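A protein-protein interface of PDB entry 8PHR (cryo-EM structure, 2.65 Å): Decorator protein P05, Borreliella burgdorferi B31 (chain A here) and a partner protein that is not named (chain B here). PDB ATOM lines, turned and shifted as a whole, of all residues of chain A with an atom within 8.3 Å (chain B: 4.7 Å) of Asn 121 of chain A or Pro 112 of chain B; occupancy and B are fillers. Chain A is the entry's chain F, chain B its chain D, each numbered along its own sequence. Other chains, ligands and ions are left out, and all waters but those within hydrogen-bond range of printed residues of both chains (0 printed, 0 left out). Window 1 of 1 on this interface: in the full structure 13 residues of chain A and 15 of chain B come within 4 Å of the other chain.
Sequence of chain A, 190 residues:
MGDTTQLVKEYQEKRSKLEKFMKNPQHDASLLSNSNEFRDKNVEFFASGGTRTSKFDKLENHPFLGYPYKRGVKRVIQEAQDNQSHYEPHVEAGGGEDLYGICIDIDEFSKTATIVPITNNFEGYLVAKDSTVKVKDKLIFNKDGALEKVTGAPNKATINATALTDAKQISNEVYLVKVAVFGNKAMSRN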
ATOM      1  N   ARG A  52     -23.382   9.838 -20.931  1.00  0.00           N
ATOM      2  CA  ARG A  52     -24.629  10.239 -20.293  1.00  0.00           C
ATOM      3  C   ARG A  52     -25.684  10.437 -21.369  1.00  0.00           C
ATOM      4  O   ARG A  52     -25.469  11.192 -22.322  1.00  0.00           O
ATOM      5  CB  ARG A  52     -24.445  11.521 -19.474  1.00  0.00           C
ATOM      6  CG  ARG A  52     -23.360  11.428 -18.414  1.00  0.00           C
ATOM      7  CD  ARG A  52     -23.629  12.376 -17.258  1.00  0.00           C
ATOM      8  NE  ARG A  52     -22.678  12.189 -16.168  1.00  0.00           N
ATOM      9  CZ  ARG A  52     -22.777  12.767 -14.979  1.00  0.00           C
ATOM     10  NH1 ARG A  52     -23.777  13.581 -14.687  1.00  0.00           N
ATOM     11  NH2 ARG A  52     -21.847  12.522 -14.060  1.00  0.00           N
ATOM     12  N   THR A  53     -26.820   9.760 -21.216  1.00  0.00           N
ATOM     13  CA  THR A  53     -27.879   9.771 -22.215  1.00  0.00           C
ATOM     14  C   THR A  53     -29.210  10.090 -21.552  1.00  0.00           C
ATOM     15  O   THR A  53     -29.506   9.591 -20.462  1.00  0.00           O
ATOM     16  CB  THR A  53     -27.967   8.422 -22.945  1.00  0.00           C
ATOM     17  OG1 THR A  53     -26.682   8.080 -23.479  1.00  0.00           O
ATOM     18  CG2 THR A  53     -28.975   8.489 -24.084  1.00  0.00           C
ATOM     19  N   SER A  54     -30.006  10.923 -22.214  1.00  0.00           N
ATOM     20  CA  SER A  54     -31.333  11.285 -21.745  1.00  0.00           C
ATOM     21  C   SER A  54     -32.388  10.421 -22.426  1.00  0.00           C
ATOM     22  O   SER A  54     -32.191   9.929 -23.541  1.00  0.00           O
ATOM     23  CB  SER A  54     -31.623  12.764 -22.009  1.00  0.00           C
ATOM     24  OG  SER A  54     -33.013  13.032 -21.944  1.00  0.00           O
ATOM     25  N   PHE A  56     -35.178  11.382 -23.624  1.00  0.00           N
ATOM     26  CA  PHE A  56     -35.834  12.110 -24.709  1.00  0.00           C
ATOM     27  C   PHE A  56     -34.845  12.565 -25.775  1.00  0.00           C
ATOM     28  O   PHE A  56     -34.990  13.648 -26.350  1.00  0.00           O
ATOM     29  CB  PHE A  56     -36.606  13.300 -24.148  1.00  0.00           C
ATOM     30  CG  PHE A  56     -37.500  12.949 -22.994  1.00  0.00           C
ATOM     31  CD1 PHE A  56     -38.529  12.034 -23.152  1.00  0.00           C
ATOM     32  CD2 PHE A  56     -37.308  13.524 -21.750  1.00  0.00           C
ATOM     33  CE1 PHE A  56     -39.354  11.706 -22.092  1.00  0.00           C
ATOM     34  CE2 PHE A  56     -38.127  13.200 -20.686  1.00  0.00           C
ATOM     35  CZ  PHE A  56     -39.151  12.289 -20.857  1.00  0.00           C
ATOM     36  N   ASP A  57     -33.829  11.754 -26.058  1.00  0.00           N
ATOM     37  CA  ASP A  57     -32.862  12.058 -27.103  1.00  0.00           C
ATOM     38  C   ASP A  57     -33.366  11.556 -28.449  1.00  0.00           C
ATOM     39  O   ASP A  57     -33.980  10.488 -28.538  1.00  0.00           O
ATOM     40  CB  ASP A  57     -31.504  11.429 -26.782  1.00  0.00           C
ATOM     41  CG  ASP A  57     -30.620  12.341 -25.955  1.00  0.00           C
ATOM     42  OD1 ASP A  57     -31.016  13.502 -25.722  1.00  0.00           O
ATOM     43  OD2 ASP A  57     -29.530  11.898 -25.539  1.00  0.00           O
ATOM     44  N   LYS A  58     -33.103  12.333 -29.497  1.00  0.00           N
ATOM     45  CA  LYS A  58     -33.564  12.010 -30.841  1.00  0.00           C
ATOM     46  C   LYS A  58     -32.483  11.226 -31.578  1.00  0.00           C
ATOM     47  O   LYS A  58     -31.343  11.689 -31.696  1.00  0.00           O
ATOM     48  CB  LYS A  58     -33.924  13.283 -31.605  1.00  0.00           C
ATOM     49  CG  LYS A  58     -34.726  13.043 -32.873  1.00  0.00           C
ATOM     50  CD  LYS A  58     -34.908  14.330 -33.662  1.00  0.00           C
ATOM     51  CE  LYS A  58     -36.069  14.220 -34.637  1.00  0.00           C
ATOM     52  NZ  LYS A  58     -35.972  12.995 -35.479  1.00  0.00           N
ATOM     53  N   ILE A 102     -23.931  13.377 -35.711  1.00  0.00           N
ATOM     54  CA  ILE A 102     -22.823  12.528 -35.278  1.00  0.00           C
ATOM     55  C   ILE A 102     -23.313  11.094 -35.137  1.00  0.00           C
ATOM     56  O   ILE A 102     -24.385  10.843 -34.578  1.00  0.00           O
ATOM     57  CB  ILE A 102     -22.195  13.033 -33.960  1.00  0.00           C
ATOM     58  CG1 ILE A 102     -23.269  13.226 -32.889  1.00  0.00           C
ATOM     59  CG2 ILE A 102     -21.412  14.319 -34.191  1.00  0.00           C
ATOM     60  CD1 ILE A 102     -22.710  13.561 -31.535  1.00  0.00           C
ATOM     61  N   VAL A 116     -27.199  11.108 -33.975  1.00  0.00           N
ATOM     62  CA  VAL A 116     -27.776  12.179 -33.169  1.00  0.00           C
ATOM     63  C   VAL A 116     -27.648  13.469 -33.969  1.00  0.00           C
ATOM     64  O   VAL A 116     -26.520  13.841 -34.347  1.00  0.00           O
ATOM     65  CB  VAL A 116     -27.072  12.306 -31.812  1.00  0.00           C
ATOM     66  CG1 VAL A 116     -27.757  13.367 -30.958  1.00  0.00           C
ATOM     67  CG2 VAL A 116     -27.031  10.967 -31.100  1.00  0.00           C
ATOM     68  N   PRO A 117     -28.748  14.150 -34.284  1.00  0.00           N
ATOM     69  CA  PRO A 117     -28.655  15.402 -35.042  1.00  0.00           C
ATOM     70  C   PRO A 117     -27.972  16.492 -34.232  1.00  0.00           C
ATOM     71  O   PRO A 117     -27.946  16.473 -33.000  1.00  0.00           O
ATOM     72  CB  PRO A 117     -30.118  15.762 -35.327  1.00  0.00           C
ATOM     73  CG  PRO A 117     -30.882  14.486 -35.129  1.00  0.00           C
ATOM     74  CD  PRO A 117     -30.146  13.748 -34.054  1.00  0.00           C
ATOM     75  N   ILE A 118     -27.409  17.460 -34.959  1.00  0.00           N
ATOM     76  CA  ILE A 118     -26.715  18.570 -34.318  1.00  0.00           C
ATOM     77  C   ILE A 118     -27.660  19.413 -33.472  1.00  0.00           C
ATOM     78  O   ILE A 118     -27.206  20.167 -32.605  1.00  0.00           O
ATOM     79  CB  ILE A 118     -25.995  19.432 -35.378  1.00  0.00           C
ATOM     80  CG1 ILE A 118     -24.822  20.184 -34.746  1.00  0.00           C
ATOM     81  CG2 ILE A 118     -26.965  20.402 -36.035  1.00  0.00           C
ATOM     82  CD1 ILE A 118     -23.794  19.278 -34.109  1.00  0.00           C
ATOM     83  N   THR A 119     -28.972  19.304 -33.701  1.00  0.00           N
ATOM     84  CA  THR A 119     -29.935  20.020 -32.871  1.00  0.00           C
ATOM     85  C   THR A 119     -29.938  19.527 -31.431  1.00  0.00           C
ATOM     86  O   THR A 119     -30.355  20.270 -30.537  1.00  0.00           O
ATOM     87  CB  THR A 119     -31.342  19.888 -33.454  1.00  0.00           C
ATOM     88  OG1 THR A 119     -31.840  18.567 -33.212  1.00  0.00           O
ATOM     89  CG2 THR A 119     -31.322  20.145 -34.947  1.00  0.00           C
ATOM     90  N   ASN A 120     -29.489  18.302 -31.189  1.00  0.00           N
ATOM     91  CA  ASN A 120     -29.429  17.735 -29.853  1.00  0.00           C
ATOM     92  C   ASN A 120     -28.005  17.807 -29.313  1.00  0.00           C
ATOM     93  O   ASN A 120     -27.034  17.937 -30.064  1.00  0.00           O
ATOM     94  CB  ASN A 120     -29.918  16.283 -29.860  1.00  0.00           C
ATOM     95  CG  ASN A 120     -30.440  15.836 -28.510  1.00  0.00           C
ATOM     96  OD1 ASN A 120     -30.367  16.576 -27.528  1.00  0.00           O
ATOM     97  ND2 ASN A 120     -30.975  14.623 -28.454  1.00  0.00           N
ATOM     98  N   ASN A 121     -27.890  17.722 -27.991  1.00  0.00           N
ATOM     99  CA  ASN A 121     -26.602  17.770 -27.319  1.00  0.00           C
ATOM    100  C   ASN A 121     -26.155  16.361 -26.953  1.00  0.00           C
ATOM    101  O   ASN A 121     -26.973  15.514 -26.581  1.00  0.00           O
ATOM    102  CB  ASN A 121     -26.664  18.646 -26.067  1.00  0.00           C
ATOM    103  CG  ASN A 121     -27.611  18.101 -25.022  1.00  0.00           C
ATOM    104  OD1 ASN A 121     -28.804  17.938 -25.276  1.00  0.00           O
ATOM    105  ND2 ASN A 121     -27.085  17.814 -23.836  1.00  0.00           N
ATOM    106  N   PHE A 122     -24.852  16.118 -27.067  1.00  0.00           N
ATOM    107  CA  PHE A 122     -24.278  14.801 -26.850  1.00  0.00           C
ATOM    108  C   PHE A 122     -23.040  14.919 -25.973  1.00  0.00           C
ATOM    109  O   PHE A 122     -22.338  15.932 -25.996  1.00  0.00           O
ATOM    110  CB  PHE A 122     -23.917  14.128 -28.183  1.00  0.00           C
ATOM    111  CG  PHE A 122     -23.264  12.785 -28.032  1.00  0.00           C
ATOM    112  CD1 PHE A 122     -24.006  11.681 -27.648  1.00  0.00           C
ATOM    113  CD2 PHE A 122     -21.908  12.626 -28.267  1.00  0.00           C
ATOM    114  CE1 PHE A 122     -23.411  10.443 -27.507  1.00  0.00           C
ATOM    115  CE2 PHE A 122     -21.306  11.391 -28.129  1.00  0.00           C
ATOM    116  CZ  PHE A 122     -22.058  10.298 -27.747  1.00  0.00           C
ATOM    117  N   GLU A 123     -22.785  13.874 -25.190  1.00  0.00           N
ATOM    118  CA  GLU A 123     -21.599  13.799 -24.339  1.00  0.00           C
ATOM    119  C   GLU A 123     -21.037  12.390 -24.461  1.00  0.00           C
ATOM    120  O   GLU A 123     -21.673  11.432 -24.011  1.00  0.00           O
ATOM    121  CB  GLU A 123     -21.934  14.125 -22.882  1.00  0.00           C
ATOM    122  CG  GLU A 123     -22.354  15.564 -22.637  1.00  0.00           C
ATOM    123  CD  GLU A 123     -22.696  15.831 -21.184  1.00  0.00           C
ATOM    124  OE1 GLU A 123     -22.724  14.865 -20.391  1.00  0.00           O
ATOM    125  OE2 GLU A 123     -22.937  17.005 -20.835  1.00  0.00           O
ATOM    126  N   GLY A 124     -19.859  12.255 -25.057  1.00  0.00           N
ATOM    127  CA  GLY A 124     -19.307  10.924 -25.234  1.00  0.00           C
ATOM    128  C   GLY A 124     -17.969  10.959 -25.934  1.00  0.00           C
ATOM    129  O   GLY A 124     -17.415  12.023 -26.209  1.00  0.00           O
ATOM    130  N   ASN A 160     -19.908  24.330 -31.358  1.00  0.00           N
ATOM    131  CA  ASN A 160     -19.244  24.525 -30.073  1.00  0.00           C
ATOM    132  C   ASN A 160     -19.057  23.173 -29.394  1.00  0.00           C
ATOM    133  O   ASN A 160     -20.015  22.582 -28.884  1.00  0.00           O
ATOM    134  CB  ASN A 160     -20.032  25.498 -29.196  1.00  0.00           C
ATOM    135  CG  ASN A 160     -21.525  25.218 -29.194  1.00  0.00           C
ATOM    136  OD1 ASN A 160     -21.978  24.175 -29.658  1.00  0.00           O
ATOM    137  ND2 ASN A 160     -22.301  26.166 -28.678  1.00  0.00           N
ATOM    138  N   VAL A 179     -15.906  14.309 -25.365  1.00  0.00           N
ATOM    139  CA  VAL A 179     -16.295  15.636 -25.817  1.00  0.00           C
ATOM    140  C   VAL A 179     -17.791  15.809 -25.594  1.00  0.00           C
ATOM    141  O   VAL A 179     -18.568  14.854 -25.729  1.00  0.00           O
ATOM    142  CB  VAL A 179     -15.931  15.856 -27.303  1.00  0.00           C
ATOM    143  CG1 VAL A 179     -16.350  17.244 -27.772  1.00  0.00           C
ATOM    144  CG2 VAL A 179     -14.441  15.655 -27.519  1.00  0.00           C
ATOM    145  N   ALA A 180     -18.183  17.024 -25.216  1.00  0.00           N
ATOM    146  CA  ALA A 180     -19.580  17.424 -25.109  1.00  0.00           C
ATOM    147  C   ALA A 180     -19.876  18.438 -26.206  1.00  0.00           C
ATOM    148  O   ALA A 180     -19.287  19.525 -26.228  1.00  0.00           O
ATOM    149  CB  ALA A 180     -19.880  18.013 -23.732  1.00  0.00           C
ATOM    150  N   VAL A 181     -20.783  18.080 -27.111  1.00  0.00           N
ATOM    151  CA  VAL A 181     -21.213  18.944 -28.203  1.00  0.00           C
ATOM    152  C   VAL A 181     -22.616  19.438 -27.884  1.00  0.00           C
ATOM    153  O   VAL A 181     -23.519  18.633 -27.623  1.00  0.00           O
ATOM    154  CB  VAL A 181     -21.180  18.208 -29.553  1.00  0.00           C
ATOM    155  CG1 VAL A 181     -21.410  19.184 -30.695  1.00  0.00           C
ATOM    156  CG2 VAL A 181     -19.856  17.479 -29.727  1.00  0.00           C
ATOM    157  N   PHE A 182     -22.798  20.755 -27.902  1.00  0.00           N
ATOM    158  CA  PHE A 182     -24.043  21.383 -27.471  1.00  0.00           C
ATOM    159  C   PHE A 182     -24.490  22.449 -28.468  1.00  0.00           C
ATOM    160  O   PHE A 182     -24.865  23.565 -28.104  1.00  0.00           O
ATOM    161  CB  PHE A 182     -23.895  21.945 -26.054  1.00  0.00           C
ATOM    162  CG  PHE A 182     -22.789  22.957 -25.898  1.00  0.00           C
ATOM    163  CD1 PHE A 182     -21.466  22.550 -25.795  1.00  0.00           C
ATOM    164  CD2 PHE A 182     -23.073  24.311 -25.814  1.00  0.00           C
ATOM    165  CE1 PHE A 182     -20.450  23.475 -25.641  1.00  0.00           C
ATOM    166  CE2 PHE A 182     -22.059  25.238 -25.658  1.00  0.00           C
ATOM    167  CZ  PHE A 182     -20.747  24.819 -25.572  1.00  0.00           C
ATOM    168  N   GLY A 183     -24.474  22.102 -29.753  1.00  0.00           N
ATOM    169  CA  GLY A 183     -25.073  22.955 -30.762  1.00  0.00           C
ATOM    170  C   GLY A 183     -24.097  23.623 -31.708  1.00  0.00           C
ATOM    171  O   GLY A 183     -23.023  23.086 -31.995  1.00  0.00           O
ATOM    172  N   LYS B  58     -35.163  18.227 -22.086  1.00  0.00           N
ATOM    173  CA  LYS B  58     -33.942  17.641 -21.550  1.00  0.00           C
ATOM    174  C   LYS B  58     -33.376  18.543 -20.461  1.00  0.00           C
ATOM    175  O   LYS B  58     -33.189  19.745 -20.676  1.00  0.00           O
ATOM    176  CB  LYS B  58     -32.906  17.429 -22.654  1.00  0.00           C
ATOM    177  CG  LYS B  58     -31.677  16.654 -22.211  1.00  0.00           C
ATOM    178  CD  LYS B  58     -30.778  16.334 -23.392  1.00  0.00           C
ATOM    179  CE  LYS B  58     -29.546  15.555 -22.959  1.00  0.00           C
ATOM    180  NZ  LYS B  58     -28.690  15.180 -24.117  1.00  0.00           N
ATOM    181  N   GLU B  60     -30.415  18.553 -17.075  1.00  0.00           N
ATOM    182  CA  GLU B  60     -29.230  17.898 -16.532  1.00  0.00           C
ATOM    183  C   GLU B  60     -28.835  18.556 -15.219  1.00  0.00           C
ATOM    184  O   GLU B  60     -28.751  19.783 -15.142  1.00  0.00           O
ATOM    185  CB  GLU B  60     -28.063  17.971 -17.524  1.00  0.00           C
ATOM    186  CG  GLU B  60     -28.322  17.283 -18.854  1.00  0.00           C
ATOM    187  CD  GLU B  60     -27.335  17.699 -19.927  1.00  0.00           C
ATOM    188  OE1 GLU B  60     -26.532  18.622 -19.673  1.00  0.00           O
ATOM    189  OE2 GLU B  60     -27.360  17.104 -21.024  1.00  0.00           O
ATOM    190  N   TYR B  95     -23.509  27.749 -22.021  1.00  0.00           N
ATOM    191  CA  TYR B  95     -23.819  26.341 -22.222  1.00  0.00           C
ATOM    192  C   TYR B  95     -25.279  25.996 -21.981  1.00  0.00           C
ATOM    193  O   TYR B  95     -25.799  25.089 -22.638  1.00  0.00           O
ATOM    194  CB  TYR B  95     -22.941  25.469 -21.307  1.00  0.00           C
ATOM    195  CG  TYR B  95     -23.365  24.018 -21.232  1.00  0.00           C
ATOM    196  CD1 TYR B  95     -23.199  23.169 -22.319  1.00  0.00           C
ATOM    197  CD2 TYR B  95     -23.927  23.498 -20.074  1.00  0.00           C
ATOM    198  CE1 TYR B  95     -23.582  21.843 -22.255  1.00  0.00           C
ATOM    199  CE2 TYR B  95     -24.315  22.173 -20.001  1.00  0.00           C
ATOM    200  CZ  TYR B  95     -24.141  21.352 -21.094  1.00  0.00           C
ATOM    201  OH  TYR B  95     -24.524  20.032 -21.025  1.00  0.00           O
ATOM    202  N   GLY B  96     -25.955  26.690 -21.075  1.00  0.00           N
ATOM    203  CA  GLY B  96     -27.349  26.398 -20.812  1.00  0.00           C
ATOM    204  C   GLY B  96     -27.954  27.424 -19.882  1.00  0.00           C
ATOM    205  O   GLY B  96     -27.345  28.450 -19.574  1.00  0.00           O
ATOM    206  N   VAL B 110     -30.009  22.347 -15.265  1.00  0.00           N
ATOM    207  CA  VAL B 110     -29.708  23.173 -16.425  1.00  0.00           C
ATOM    208  C   VAL B 110     -30.434  22.595 -17.629  1.00  0.00           C
ATOM    209  O   VAL B 110     -30.403  21.379 -17.857  1.00  0.00           O
ATOM    210  CB  VAL B 110     -28.193  23.248 -16.684  1.00  0.00           C
ATOM    211  CG1 VAL B 110     -27.906  23.934 -18.012  1.00  0.00           C
ATOM    212  CG2 VAL B 110     -27.492  23.965 -15.539  1.00  0.00           C
ATOM    213  N   ILE B 111     -31.106  23.463 -18.375  1.00  0.00           N
ATOM    214  CA  ILE B 111     -31.641  23.135 -19.691  1.00  0.00           C
ATOM    215  C   ILE B 111     -30.599  23.547 -20.724  1.00  0.00           C
ATOM    216  O   ILE B 111     -30.189  24.719 -20.735  1.00  0.00           O
ATOM    217  CB  ILE B 111     -32.981  23.839 -19.948  1.00  0.00           C
ATOM    218  CG1 ILE B 111     -34.027  23.374 -18.933  1.00  0.00           C
ATOM    219  CG2 ILE B 111     -33.454  23.577 -21.371  1.00  0.00           C
ATOM    220  CD1 ILE B 111     -35.431  23.849 -19.234  1.00  0.00           C
ATOM    221  N   PRO B 112     -30.130  22.637 -21.574  1.00  0.00           N
ATOM    222  CA  PRO B 112     -29.090  22.992 -22.544  1.00  0.00           C
ATOM    223  C   PRO B 112     -29.581  24.022 -23.548  1.00  0.00           C
ATOM    224  O   PRO B 112     -30.778  24.168 -23.804  1.00  0.00           O
ATOM    225  CB  PRO B 112     -28.770  21.660 -23.232  1.00  0.00           C
ATOM    226  CG  PRO B 112     -29.243  20.610 -22.280  1.00  0.00           C
ATOM    227  CD  PRO B 112     -30.442  21.197 -21.598  1.00  0.00           C
ATOM    228  N   ILE B 113     -28.617  24.753 -24.115  1.00  0.00           N
ATOM    229  CA  ILE B 113     -28.934  25.767 -25.116  1.00  0.00           C
ATOM    230  C   ILE B 113     -29.580  25.131 -26.341  1.00  0.00           C
ATOM    231  O   ILE B 113     -30.322  25.793 -27.078  1.00  0.00           O
ATOM    232  CB  ILE B 113     -27.667  26.565 -25.485  1.00  0.00           C
ATOM    233  CG1 ILE B 113     -28.025  27.796 -26.320  1.00  0.00           C
ATOM    234  CG2 ILE B 113     -26.667  25.684 -26.221  1.00  0.00           C
ATOM    235  CD1 ILE B 113     -28.880  28.802 -25.585  1.00  0.00           C
ATOM    236  N   THR B 114     -29.318  23.843 -26.579  1.00  0.00           N
ATOM    237  CA  THR B 114     -29.956  23.137 -27.684  1.00  0.00           C
ATOM    238  C   THR B 114     -31.458  22.986 -27.484  1.00  0.00           C
ATOM    239  O   THR B 114     -32.176  22.720 -28.455  1.00  0.00           O
ATOM    240  CB  THR B 114     -29.328  21.754 -27.862  1.00  0.00           C
ATOM    241  OG1 THR B 114     -29.598  20.951 -26.706  1.00  0.00           O
ATOM    242  CG2 THR B 114     -27.826  21.870 -28.053  1.00  0.00           C
ATOM    243  N   ASN B 115     -31.947  23.146 -26.258  1.00  0.00           N
ATOM    244  CA  ASN B 115     -33.365  23.048 -25.951  1.00  0.00           C
ATOM    245  C   ASN B 115     -33.903  24.426 -25.589  1.00  0.00           C
ATOM    246  O   ASN B 115     -33.282  25.162 -24.817  1.00  0.00           O
ATOM    247  CB  ASN B 115     -33.607  22.067 -24.800  1.00  0.00           C
ATOM    248  CG  ASN B 115     -35.026  21.535 -24.775  1.00  0.00           C
ATOM    249  OD1 ASN B 115     -35.987  22.299 -24.692  1.00  0.00           O
ATOM    250  ND2 ASN B 115     -35.164  20.217 -24.847  1.00  0.00           N
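NZ of Lys 58 of chain B lies within salt-bridge range of OD1 of Asp 57 of chain A, 3.3 Å away. OE2 of Glu 60 of chain B lies within hydrogen-bond range of ND2 of Asn 121 of chain A, at 2.9 Å. OE2 of Glu 123 of chain A sits at hydrogen-bond distance from OH of Tyr 95 of chain B (3.4 Å). The side-chain amide oxygen (OD1) of Asn 121 of chain A lies within hydrogen-bond range of the side-chain hydroxyl (OG1) of Thr 114 of chain B (3.4 Å). The side-chain amide oxygen of Asn 121 of chain A lies within hydrogen-bond range of the side-chain amino group of Lys 58 of chain B.
The backbone carbonyl oxygen (O) of Tyr 95 of chain B lies within hydrogen-bond range of the backbone NH (N) of Ile 113 of chain B, at 3.2 Å. The backbone NH (N) of Ser 54 of chain A is in hydrogen-bond range of the side-chain carboxylate (OD2) of Asp 57 of chain A (3.5 Å). The side-chain amide oxygen of Asn 160 of chain A lies close to the backbone carbonyl oxygen of Phe 182 of chain A, at 3.3 Å. The backbone NH of Lys 58 of chain B sits close to the side-chain amide nitrogen of Asn 115 of chain B, 3.4 Å away. The side-chain amide oxygen (OD1) of Asn 120 of chain A sits close to the side-chain amide oxygen (OD1) of Asn 121 of chain A (3.1 Å). The side-chain amide nitrogen (ND2) of Asn 120 of chain A sits at hydrogen-bond distance from the side-chain carboxylate (OD1) of Asp 57 of chain A, at 3.0 Å.
Among the printed residues, merely in contact across the chains: Ser 54 of chain A with Lys 58 of chain B (3.6 Å), Thr 119 of chain A with Thr 114 of chain B (3.2 Å), Asn 121 of chain A with Pro 112 of chain B (3.9 Å), Phe 182 of chain A with Tyr 95 of chain B (3.6 Å), Phe 182 of chain A with Ile 113 of chain B (3.4 Å), Phe 182 of chain A with Thr 114 of chain B (3.4 Å) and Gly 183 of chain A with Thr 114 of chain B (3.8 Å).
Arg 52 of chain A touches none of the printed residues of chain B. Printed residues of chain B within 4 Å of Ser 54 of chain A: Lys 58. Of chain B, only Lys 58 (3.0 Å), Glu 60 (2.9 Å), Pro 112 (3.9 Å) and Thr 114 (3.4 Å) come within 4 Å of Asn 121 of chain A. Of the printed residues of chain B, Glu 123 of chain A touches Tyr 95 (3.4 Å). Val 110 of chain B touches none of the printed residues of chain A. Pro 112 of chain B touches just one residue of chain A: Asn 121. Of the printed residues of chain A, Ile 113 of chain B touches Phe 182. The nearest residue of chain B that does not touch Asn 121 of chain A is Tyr 95 of chain B (4.4 Å). The nearest residue of chain A that does not touch Pro 112 of chain B is Phe 182 of chain A (5.6 Å). The nearest printed residue of chain B that does not touch Asp 57 of chain A is Glu 60 of chain B (7.0 Å).
Printed residues of chain A that touch a printed residue of chain B: Ser 54, Asp 57, Thr 119, Asn 121, Glu 123, Phe 182 and Gly 183. Hydrophobic or aromatic side chains of chain A that line the printed part of chain B: Phe 182. Among the printed residues, 12 pairs touch across the chains. Among the printed residues, Asp or Glu carboxylates within 4 Å of a Lys or Arg side-chain nitrogen of the other chain: Asp 57 of chain A with Lys 58 of chain B.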
